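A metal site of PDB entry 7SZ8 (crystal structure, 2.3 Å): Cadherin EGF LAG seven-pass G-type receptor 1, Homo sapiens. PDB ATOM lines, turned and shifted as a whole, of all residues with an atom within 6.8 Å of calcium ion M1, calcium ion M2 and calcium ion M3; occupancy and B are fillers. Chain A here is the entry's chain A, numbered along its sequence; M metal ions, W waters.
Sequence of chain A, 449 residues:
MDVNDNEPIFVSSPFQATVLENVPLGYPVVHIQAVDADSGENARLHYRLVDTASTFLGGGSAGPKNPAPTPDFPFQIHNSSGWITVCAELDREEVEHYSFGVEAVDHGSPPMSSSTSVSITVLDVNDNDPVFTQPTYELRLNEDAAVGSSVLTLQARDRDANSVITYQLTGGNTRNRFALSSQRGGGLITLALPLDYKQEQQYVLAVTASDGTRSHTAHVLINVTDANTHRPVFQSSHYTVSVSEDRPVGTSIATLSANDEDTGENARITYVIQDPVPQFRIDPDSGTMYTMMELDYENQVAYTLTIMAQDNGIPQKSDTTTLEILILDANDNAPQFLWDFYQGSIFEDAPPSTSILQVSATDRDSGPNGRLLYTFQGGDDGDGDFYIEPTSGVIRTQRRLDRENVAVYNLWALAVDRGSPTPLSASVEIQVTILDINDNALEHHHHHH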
ATOM      1  N   GLU A 245     -22.076  -7.150  30.950  1.00  0.00           N
ATOM      2  CA  GLU A 245     -23.052  -7.631  29.932  1.00  0.00           C
ATOM      3  C   GLU A 245     -22.872  -9.153  29.688  1.00  0.00           C
ATOM      4  O   GLU A 245     -23.780  -9.760  29.072  1.00  0.00           O
ATOM      5  CB  GLU A 245     -22.923  -6.764  28.691  1.00  0.00           C
ATOM      6  CG  GLU A 245     -21.690  -7.083  27.877  1.00  0.00           C
ATOM      7  CD  GLU A 245     -21.670  -6.387  26.533  1.00  0.00           C
ATOM      8  OE1 GLU A 245     -20.628  -5.779  26.203  1.00  0.00           O
ATOM      9  OE2 GLU A 245     -22.692  -6.462  25.817  1.00  0.00           O
ATOM     10  N   LEU A 295     -28.125  -9.515  28.904  1.00  0.00           N
ATOM     11  CA  LEU A 295     -27.927  -8.038  28.883  1.00  0.00           C
ATOM     12  C   LEU A 295     -27.000  -7.701  27.722  1.00  0.00           C
ATOM     13  O   LEU A 295     -26.118  -8.538  27.457  1.00  0.00           O
ATOM     14  CB  LEU A 295     -27.309  -7.616  30.212  1.00  0.00           C
ATOM     15  CG  LEU A 295     -28.215  -7.858  31.411  1.00  0.00           C
ATOM     16  CD1 LEU A 295     -27.459  -7.720  32.739  1.00  0.00           C
ATOM     17  CD2 LEU A 295     -29.416  -6.927  31.344  1.00  0.00           C
ATOM     18  N   ASP A 296     -27.198  -6.561  27.061  1.00  0.00           N
ATOM     19  CA  ASP A 296     -26.309  -6.123  25.948  1.00  0.00           C
ATOM     20  C   ASP A 296     -25.943  -4.654  26.125  1.00  0.00           C
ATOM     21  O   ASP A 296     -26.790  -3.772  25.855  1.00  0.00           O
ATOM     22  CB  ASP A 296     -26.911  -6.406  24.574  1.00  0.00           C
ATOM     23  CG  ASP A 296     -26.039  -6.095  23.348  1.00  0.00           C
ATOM     24  OD1 ASP A 296     -24.927  -5.536  23.493  1.00  0.00           O
ATOM     25  OD2 ASP A 296     -26.510  -6.371  22.230  1.00  0.00           O
ATOM     26  N   TYR A 297     -24.691  -4.411  26.502  1.00  0.00           N
ATOM     27  CA  TYR A 297     -24.115  -3.051  26.583  1.00  0.00           C
ATOM     28  C   TYR A 297     -24.382  -2.263  25.298  1.00  0.00           C
ATOM     29  O   TYR A 297     -24.629  -1.041  25.399  1.00  0.00           O
ATOM     30  CB  TYR A 297     -22.614  -3.089  26.886  1.00  0.00           C
ATOM     31  CG  TYR A 297     -22.016  -1.734  27.112  1.00  0.00           C
ATOM     32  CD1 TYR A 297     -21.554  -0.998  26.038  1.00  0.00           C
ATOM     33  CD2 TYR A 297     -21.937  -1.172  28.375  1.00  0.00           C
ATOM     34  CE1 TYR A 297     -21.012   0.260  26.215  1.00  0.00           C
ATOM     35  CE2 TYR A 297     -21.379   0.080  28.575  1.00  0.00           C
ATOM     36  CZ  TYR A 297     -20.914   0.798  27.484  1.00  0.00           C
ATOM     37  OH  TYR A 297     -20.359   2.049  27.622  1.00  0.00           O
ATOM     38  N   GLU A 298     -24.299  -2.907  24.117  1.00  0.00           N
ATOM     39  CA  GLU A 298     -24.438  -2.205  22.802  1.00  0.00           C
ATOM     40  C   GLU A 298     -25.898  -1.781  22.560  1.00  0.00           C
ATOM     41  O   GLU A 298     -26.136  -1.049  21.597  1.00  0.00           O
ATOM     42  CB  GLU A 298     -23.903  -3.072  21.657  1.00  0.00           C
ATOM     43  CG  GLU A 298     -22.369  -3.134  21.595  1.00  0.00           C
ATOM     44  CD  GLU A 298     -21.643  -3.686  22.824  1.00  0.00           C
ATOM     45  OE1 GLU A 298     -21.846  -4.865  23.185  1.00  0.00           O
ATOM     46  OE2 GLU A 298     -20.875  -2.953  23.399  1.00  0.00           O
ATOM     47  N   ASN A 299     -26.822  -2.206  23.422  1.00  0.00           N
ATOM     48  CA  ASN A 299     -28.282  -1.949  23.313  1.00  0.00           C
ATOM     49  C   ASN A 299     -28.799  -0.993  24.416  1.00  0.00           C
ATOM     50  O   ASN A 299     -29.551  -0.063  24.052  1.00  0.00           O
ATOM     51  CB  ASN A 299     -29.058  -3.259  23.322  1.00  0.00           C
ATOM     52  CG  ASN A 299     -30.542  -3.011  23.318  1.00  0.00           C
ATOM     53  OD1 ASN A 299     -31.224  -3.360  24.266  1.00  0.00           O
ATOM     54  ND2 ASN A 299     -31.021  -2.353  22.270  1.00  0.00           N
ATOM     55  N   LEU A 328     -21.547  -3.052  32.358  1.00  0.00           N
ATOM     56  CA  LEU A 328     -20.121  -2.958  31.959  1.00  0.00           C
ATOM     57  C   LEU A 328     -19.927  -3.690  30.635  1.00  0.00           C
ATOM     58  O   LEU A 328     -20.389  -4.857  30.497  1.00  0.00           O
ATOM     59  CB  LEU A 328     -19.216  -3.534  33.040  1.00  0.00           C
ATOM     60  CG  LEU A 328     -19.278  -2.847  34.405  1.00  0.00           C
ATOM     61  CD1 LEU A 328     -18.181  -3.382  35.292  1.00  0.00           C
ATOM     62  CD2 LEU A 328     -19.189  -1.335  34.313  1.00  0.00           C
ATOM     63  N   ASP A 329     -19.305  -3.013  29.679  1.00  0.00           N
ATOM     64  CA  ASP A 329     -19.012  -3.548  28.328  1.00  0.00           C
ATOM     65  C   ASP A 329     -18.036  -4.734  28.437  1.00  0.00           C
ATOM     66  O   ASP A 329     -17.134  -4.689  29.242  1.00  0.00           O
ATOM     67  CB  ASP A 329     -18.512  -2.427  27.407  1.00  0.00           C
ATOM     68  CG  ASP A 329     -18.120  -2.879  26.016  1.00  0.00           C
ATOM     69  OD1 ASP A 329     -18.891  -3.647  25.388  1.00  0.00           O
ATOM     70  OD2 ASP A 329     -17.030  -2.445  25.574  1.00  0.00           O
ATOM     71  N   ALA A 330     -18.266  -5.755  27.626  1.00  0.00           N
ATOM     72  CA  ALA A 330     -17.459  -6.980  27.496  1.00  0.00           C
ATOM     73  C   ALA A 330     -16.973  -7.054  26.033  1.00  0.00           C
ATOM     74  O   ALA A 330     -17.666  -6.529  25.151  1.00  0.00           O
ATOM     75  CB  ALA A 330     -18.355  -8.139  27.880  1.00  0.00           C
ATOM     76  N   ASN A 331     -15.825  -7.691  25.771  1.00  0.00           N
ATOM     77  CA  ASN A 331     -15.299  -7.775  24.383  1.00  0.00           C
ATOM     78  C   ASN A 331     -16.081  -8.863  23.638  1.00  0.00           C
ATOM     79  O   ASN A 331     -15.532  -9.931  23.356  1.00  0.00           O
ATOM     80  CB  ASN A 331     -13.787  -7.995  24.329  1.00  0.00           C
ATOM     81  CG  ASN A 331     -13.205  -7.663  22.963  1.00  0.00           C
ATOM     82  OD1 ASN A 331     -13.745  -6.840  22.214  1.00  0.00           O
ATOM     83  ND2 ASN A 331     -12.113  -8.329  22.625  1.00  0.00           N
ATOM     84  N   ASP A 332     -17.338  -8.590  23.320  1.00  0.00           N
ATOM     85  CA  ASP A 332     -18.197  -9.566  22.608  1.00  0.00           C
ATOM     86  C   ASP A 332     -18.448  -9.060  21.186  1.00  0.00           C
ATOM     87  O   ASP A 332     -19.406  -9.505  20.572  1.00  0.00           O
ATOM     88  CB  ASP A 332     -19.468  -9.867  23.429  1.00  0.00           C
ATOM     89  CG  ASP A 332     -20.398  -8.687  23.683  1.00  0.00           C
ATOM     90  OD1 ASP A 332     -20.068  -7.515  23.253  1.00  0.00           O
ATOM     91  OD2 ASP A 332     -21.448  -8.937  24.327  1.00  0.00           O
ATOM     92  N   ASN A 333     -17.585  -8.190  20.647  1.00  0.00           N
ATOM     93  CA  ASN A 333     -17.674  -7.829  19.199  1.00  0.00           C
ATOM     94  C   ASN A 333     -16.281  -7.876  18.587  1.00  0.00           C
ATOM     95  O   ASN A 333     -15.343  -7.282  19.186  1.00  0.00           O
ATOM     96  CB  ASN A 333     -18.341  -6.466  18.966  1.00  0.00           C
ATOM     97  CG  ASN A 333     -19.827  -6.507  19.208  1.00  0.00           C
ATOM     98  OD1 ASN A 333     -20.584  -6.750  18.266  1.00  0.00           O
ATOM     99  ND2 ASN A 333     -20.271  -6.320  20.437  1.00  0.00           N
ATOM    100  N   ALA A 334     -16.184  -8.512  17.426  1.00  0.00           N
ATOM    101  CA  ALA A 334     -14.963  -8.687  16.608  1.00  0.00           C
ATOM    102  C   ALA A 334     -14.865  -7.499  15.669  1.00  0.00           C
ATOM    103  O   ALA A 334     -15.860  -7.095  15.103  1.00  0.00           O
ATOM    104  CB  ALA A 334     -14.996  -9.986  15.835  1.00  0.00           C
ATOM    105  N   PRO A 335     -13.664  -6.918  15.438  1.00  0.00           N
ATOM    106  CA  PRO A 335     -13.531  -5.904  14.397  1.00  0.00           C
ATOM    107  C   PRO A 335     -14.072  -6.397  13.054  1.00  0.00           C
ATOM    108  O   PRO A 335     -14.177  -7.608  12.846  1.00  0.00           O
ATOM    109  CB  PRO A 335     -12.035  -5.627  14.386  1.00  0.00           C
ATOM    110  CG  PRO A 335     -11.621  -5.922  15.819  1.00  0.00           C
ATOM    111  CD  PRO A 335     -12.409  -7.166  16.162  1.00  0.00           C
ATOM    112  N   ASP A 363     -15.584  -1.552  15.353  1.00  0.00           N
ATOM    113  CA  ASP A 363     -15.799  -2.485  16.486  1.00  0.00           C
ATOM    114  C   ASP A 363     -16.881  -1.838  17.343  1.00  0.00           C
ATOM    115  O   ASP A 363     -16.676  -0.683  17.813  1.00  0.00           O
ATOM    116  CB  ASP A 363     -14.488  -2.807  17.229  1.00  0.00           C
ATOM    117  CG  ASP A 363     -14.635  -3.800  18.367  1.00  0.00           C
ATOM    118  OD1 ASP A 363     -15.715  -3.804  19.013  1.00  0.00           O
ATOM    119  OD2 ASP A 363     -13.647  -4.582  18.634  1.00  0.00           O
ATOM    120  N   ARG A 364     -17.984  -2.569  17.550  1.00  0.00           N
ATOM    121  CA  ARG A 364     -19.216  -2.022  18.173  1.00  0.00           C
ATOM    122  C   ARG A 364     -18.996  -1.825  19.680  1.00  0.00           C
ATOM    123  O   ARG A 364     -19.708  -1.016  20.273  1.00  0.00           O
ATOM    124  CB  ARG A 364     -20.415  -2.909  17.820  1.00  0.00           C
ATOM    125  CG  ARG A 364     -20.678  -3.021  16.333  1.00  0.00           C
ATOM    126  CD  ARG A 364     -21.812  -3.991  16.134  1.00  0.00           C
ATOM    127  NE  ARG A 364     -23.042  -3.495  16.760  1.00  0.00           N
ATOM    128  CZ  ARG A 364     -23.674  -4.057  17.802  1.00  0.00           C
ATOM    129  NH1 ARG A 364     -23.200  -5.149  18.380  1.00  0.00           N
ATOM    130  NH2 ARG A 364     -24.796  -3.517  18.252  1.00  0.00           N
ATOM    131  N   ASP A 365     -17.984  -2.475  20.255  1.00  0.00           N
ATOM    132  CA  ASP A 365     -17.559  -2.320  21.670  1.00  0.00           C
ATOM    133  C   ASP A 365     -17.016  -0.900  21.901  1.00  0.00           C
ATOM    134  O   ASP A 365     -16.673  -0.193  20.926  1.00  0.00           O
ATOM    135  CB  ASP A 365     -16.540  -3.410  22.044  1.00  0.00           C
ATOM    136  CG  ASP A 365     -17.111  -4.832  21.978  1.00  0.00           C
ATOM    137  OD1 ASP A 365     -18.238  -5.050  22.481  1.00  0.00           O
ATOM    138  OD2 ASP A 365     -16.422  -5.701  21.431  1.00  0.00           O
ATOM    139  N   SER A 366     -16.922  -0.496  23.171  1.00  0.00           N
ATOM    140  CA  SER A 366     -16.348   0.807  23.626  1.00  0.00           C
ATOM    141  C   SER A 366     -15.045   0.533  24.388  1.00  0.00           C
ATOM    142  O   SER A 366     -14.745  -0.666  24.641  1.00  0.00           O
ATOM    143  CB  SER A 366     -17.357   1.563  24.478  1.00  0.00           C
ATOM    144  OG  SER A 366     -18.682   1.413  23.964  1.00  0.00           O
ATOM    145  N   PRO A 368     -11.033   0.086  25.530  1.00  0.00           N
ATOM    146  CA  PRO A 368     -10.106  -0.908  24.953  1.00  0.00           C
ATOM    147  C   PRO A 368     -10.768  -1.979  24.060  1.00  0.00           C
ATOM    148  O   PRO A 368     -10.173  -2.397  23.042  1.00  0.00           O
ATOM    149  CB  PRO A 368      -9.471  -1.555  26.195  1.00  0.00           C
ATOM    150  CG  PRO A 368      -9.534  -0.483  27.291  1.00  0.00           C
ATOM    151  CD  PRO A 368     -10.773   0.325  26.965  1.00  0.00           C
ATOM    152  N   ASN A 369     -11.990  -2.382  24.402  1.00  0.00           N
ATOM    153  CA  ASN A 369     -12.725  -3.419  23.644  1.00  0.00           C
ATOM    154  C   ASN A 369     -12.943  -2.940  22.208  1.00  0.00           C
ATOM    155  O   ASN A 369     -12.997  -3.799  21.286  1.00  0.00           O
ATOM    156  CB  ASN A 369     -14.016  -3.792  24.370  1.00  0.00           C
ATOM    157  CG  ASN A 369     -13.768  -4.369  25.747  1.00  0.00           C
ATOM    158  OD1 ASN A 369     -12.782  -5.082  25.935  1.00  0.00           O
ATOM    159  ND2 ASN A 369     -14.625  -4.070  26.700  1.00  0.00           N
ATOM    160  N   GLY A 370     -13.103  -1.627  22.010  1.00  0.00           N
ATOM    161  CA  GLY A 370     -13.492  -1.003  20.723  1.00  0.00           C
ATOM    162  C   GLY A 370     -12.329  -0.373  19.965  1.00  0.00           C
ATOM    163  O   GLY A 370     -12.542  -0.059  18.786  1.00  0.00           O
ATOM    164  N   ARG A 371     -11.163  -0.228  20.613  1.00  0.00           N
ATOM    165  CA  ARG A 371      -9.934   0.454  20.111  1.00  0.00           C
ATOM    166  C   ARG A 371      -9.036  -0.513  19.301  1.00  0.00           C
ATOM    167  O   ARG A 371      -8.720  -1.591  19.792  1.00  0.00           O
ATOM    168  CB  ARG A 371      -9.150   1.000  21.298  1.00  0.00           C
ATOM    169  CG  ARG A 371      -8.103   2.044  20.932  1.00  0.00           C
ATOM    170  CD  ARG A 371      -7.510   2.627  22.181  1.00  0.00           C
ATOM    171  NE  ARG A 371      -6.112   2.999  21.972  1.00  0.00           N
ATOM    172  CZ  ARG A 371      -5.220   3.213  22.931  1.00  0.00           C
ATOM    173  NH1 ARG A 371      -5.562   3.093  24.216  1.00  0.00           N
ATOM    174  NH2 ARG A 371      -3.987   3.566  22.622  1.00  0.00           N
ATOM    175  N   LEU A 372      -8.566  -0.079  18.136  1.00  0.00           N
ATOM    176  CA  LEU A 372      -8.084  -0.961  17.035  1.00  0.00           C
ATOM    177  C   LEU A 372      -6.577  -0.770  16.757  1.00  0.00           C
ATOM    178  O   LEU A 372      -6.077   0.370  16.788  1.00  0.00           O
ATOM    179  CB  LEU A 372      -8.969  -0.683  15.811  1.00  0.00           C
ATOM    180  CG  LEU A 372     -10.418  -1.144  15.970  1.00  0.00           C
ATOM    181  CD1 LEU A 372     -11.298  -0.671  14.843  1.00  0.00           C
ATOM    182  CD2 LEU A 372     -10.498  -2.655  16.093  1.00  0.00           C
ATOM    183  N   ASP A 417      -8.646  -5.626  18.289  1.00  0.00           N
ATOM    184  CA  ASP A 417      -9.045  -4.755  19.434  1.00  0.00           C
ATOM    185  C   ASP A 417      -8.056  -4.987  20.585  1.00  0.00           C
ATOM    186  O   ASP A 417      -7.280  -5.949  20.525  1.00  0.00           O
ATOM    187  CB  ASP A 417     -10.506  -4.975  19.832  1.00  0.00           C
ATOM    188  CG  ASP A 417     -10.903  -6.376  20.256  1.00  0.00           C
ATOM    189  OD1 ASP A 417     -10.084  -7.081  20.967  1.00  0.00           O
ATOM    190  OD2 ASP A 417     -12.040  -6.773  19.887  1.00  0.00           O
ATOM    191  N   ARG A 418      -8.125  -4.140  21.613  1.00  0.00           N
ATOM    192  CA  ARG A 418      -7.307  -4.241  22.855  1.00  0.00           C
ATOM    193  C   ARG A 418      -8.159  -4.793  24.017  1.00  0.00           C
ATOM    194  O   ARG A 418      -8.013  -4.313  25.135  1.00  0.00           O
ATOM    195  CB  ARG A 418      -6.768  -2.854  23.197  1.00  0.00           C
ATOM    196  CG  ARG A 418      -6.348  -2.036  21.979  1.00  0.00           C
ATOM    197  CD  ARG A 418      -5.444  -2.761  21.006  1.00  0.00           C
ATOM    198  NE  ARG A 418      -4.871  -1.757  20.124  1.00  0.00           N
ATOM    199  CZ  ARG A 418      -3.763  -1.029  20.382  1.00  0.00           C
ATOM    200  NH1 ARG A 418      -3.054  -1.237  21.486  1.00  0.00           N
ATOM    201  NH2 ARG A 418      -3.366  -0.122  19.513  1.00  0.00           N
ATOM    202  N   GLY A 419      -9.021  -5.772  23.749  1.00  0.00           N
ATOM    203  CA  GLY A 419      -9.944  -6.324  24.756  1.00  0.00           C
ATOM    204  C   GLY A 419      -9.201  -7.228  25.711  1.00  0.00           C
ATOM    205  O   GLY A 419      -8.381  -8.047  25.235  1.00  0.00           O
ATOM    206  N   LEU A 424      -9.999  -9.751  20.345  1.00  0.00           N
ATOM    207  CA  LEU A 424     -10.619 -10.269  19.080  1.00  0.00           C
ATOM    208  C   LEU A 424      -9.987  -9.587  17.865  1.00  0.00           C
ATOM    209  O   LEU A 424      -9.455  -8.475  18.027  1.00  0.00           O
ATOM    210  CB  LEU A 424     -12.136 -10.079  19.048  1.00  0.00           C
ATOM    211  CG  LEU A 424     -12.955 -10.990  19.959  1.00  0.00           C
ATOM    212  CD1 LEU A 424     -14.350 -10.421  20.195  1.00  0.00           C
ATOM    213  CD2 LEU A 424     -13.043 -12.410  19.400  1.00  0.00           C
HETATM  214 CA    CA M   1     -23.037  -7.048  23.581  1.00  0.00          CA
HETATM  215 CA    CA M   2     -19.619  -5.274  24.126  1.00  0.00          CA
HETATM  216 CA    CA M   3     -14.223  -5.662  20.327  1.00  0.00          CA
HETATM  217  O   HOH W   1     -23.014  -7.546  21.593  1.00  0.00           O
HETATM  218  O   HOH W   2     -24.384  -8.470  24.090  1.00  0.00           O
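Of the 27 residues printed, 6 come within 4 Å of calcium ion M3.
Seven residues have an atom within 4 Å of calcium ion M2: Glu 245, Glu 298, Asp 329, Ala 330, Asp 332, Asn 333 and Asp 365.
The nearest printed residue that does not touch calcium ion M2 is Tyr 297 (4.6 Å).
The nearest printed residue that does not touch calcium ion M1 is Asn 333 (4.3 Å).
Calcium ion M2 is bound by OD1 of Asp 365 (2.2 Å), OD1 of Asp 329 (2.2 Å), OE1 of Glu 245 (2.4 Å), OD1 of Asp 332 (2.4 Å), OE1 of Glu 298 (2.5 Å), O of Ala 330 (2.5 Å) and OE2 of Glu 298 (2.7 Å).
Calcium ion M2 has seven donor atoms within binding distance.
Water W2 binds calcium ion M1 (2.0 Å).
Water W1 is bound to calcium ion M1, at 2.0 Å.
OE2 of Glu 245 is bound to calcium ion M1, at 2.3 Å.
Calcium ion M1 is bound by OD1 of Asp 296 (2.4 Å).
Calcium ion M1 is bound by the side-chain carboxylate (OE1) of Glu 298 (2.5 Å).
OD2 of Asp 332 is bound to calcium ion M1 (2.6 Å).
Calcium ion M1 has six donor atoms within binding distance.
Slightly farther from calcium ion M1 lies OD1 of Asp 332 (3.0 Å).
The side-chain amide nitrogen (ND2) of Asn 331 lies close to the backbone NH (N) of Leu 424 (3.4 Å).
OE2 of Glu 245 sits close to N of Tyr 297 (2.9 Å).
N of Ser 366 lies within hydrogen-bond range of OD2 of Asp 329, 3.1 Å away.
OD1 of Asp 417 lies within hydrogen-bond range of N of Leu 424, 2.7 Å away.
The side-chain amide oxygen (OD1) of Asn 333 lies within hydrogen-bond range of the guanidinium group (NH1) of Arg 364 (3.1 Å).
OE1 of Glu 298 lies close to ND2 of Asn 333 (3.5 Å).
The backbone carbonyl oxygen of Leu 328 is in hydrogen-bond range of the backbone NH of Glu 245, at 2.9 Å.
ND2 of Asn 369 is in hydrogen-bond range of OD2 of Asp 329, 3.1 Å away.
Calcium ion M3 is bound by OD2 of Asp 363, OD1 of Asn 331, O of Asn 333, O of Asn 369, OD2 of Asp 365, OD2 of Asp 417 and OD1 of Asp 363.
Calcium ion M3 has seven donor atoms within binding distance.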
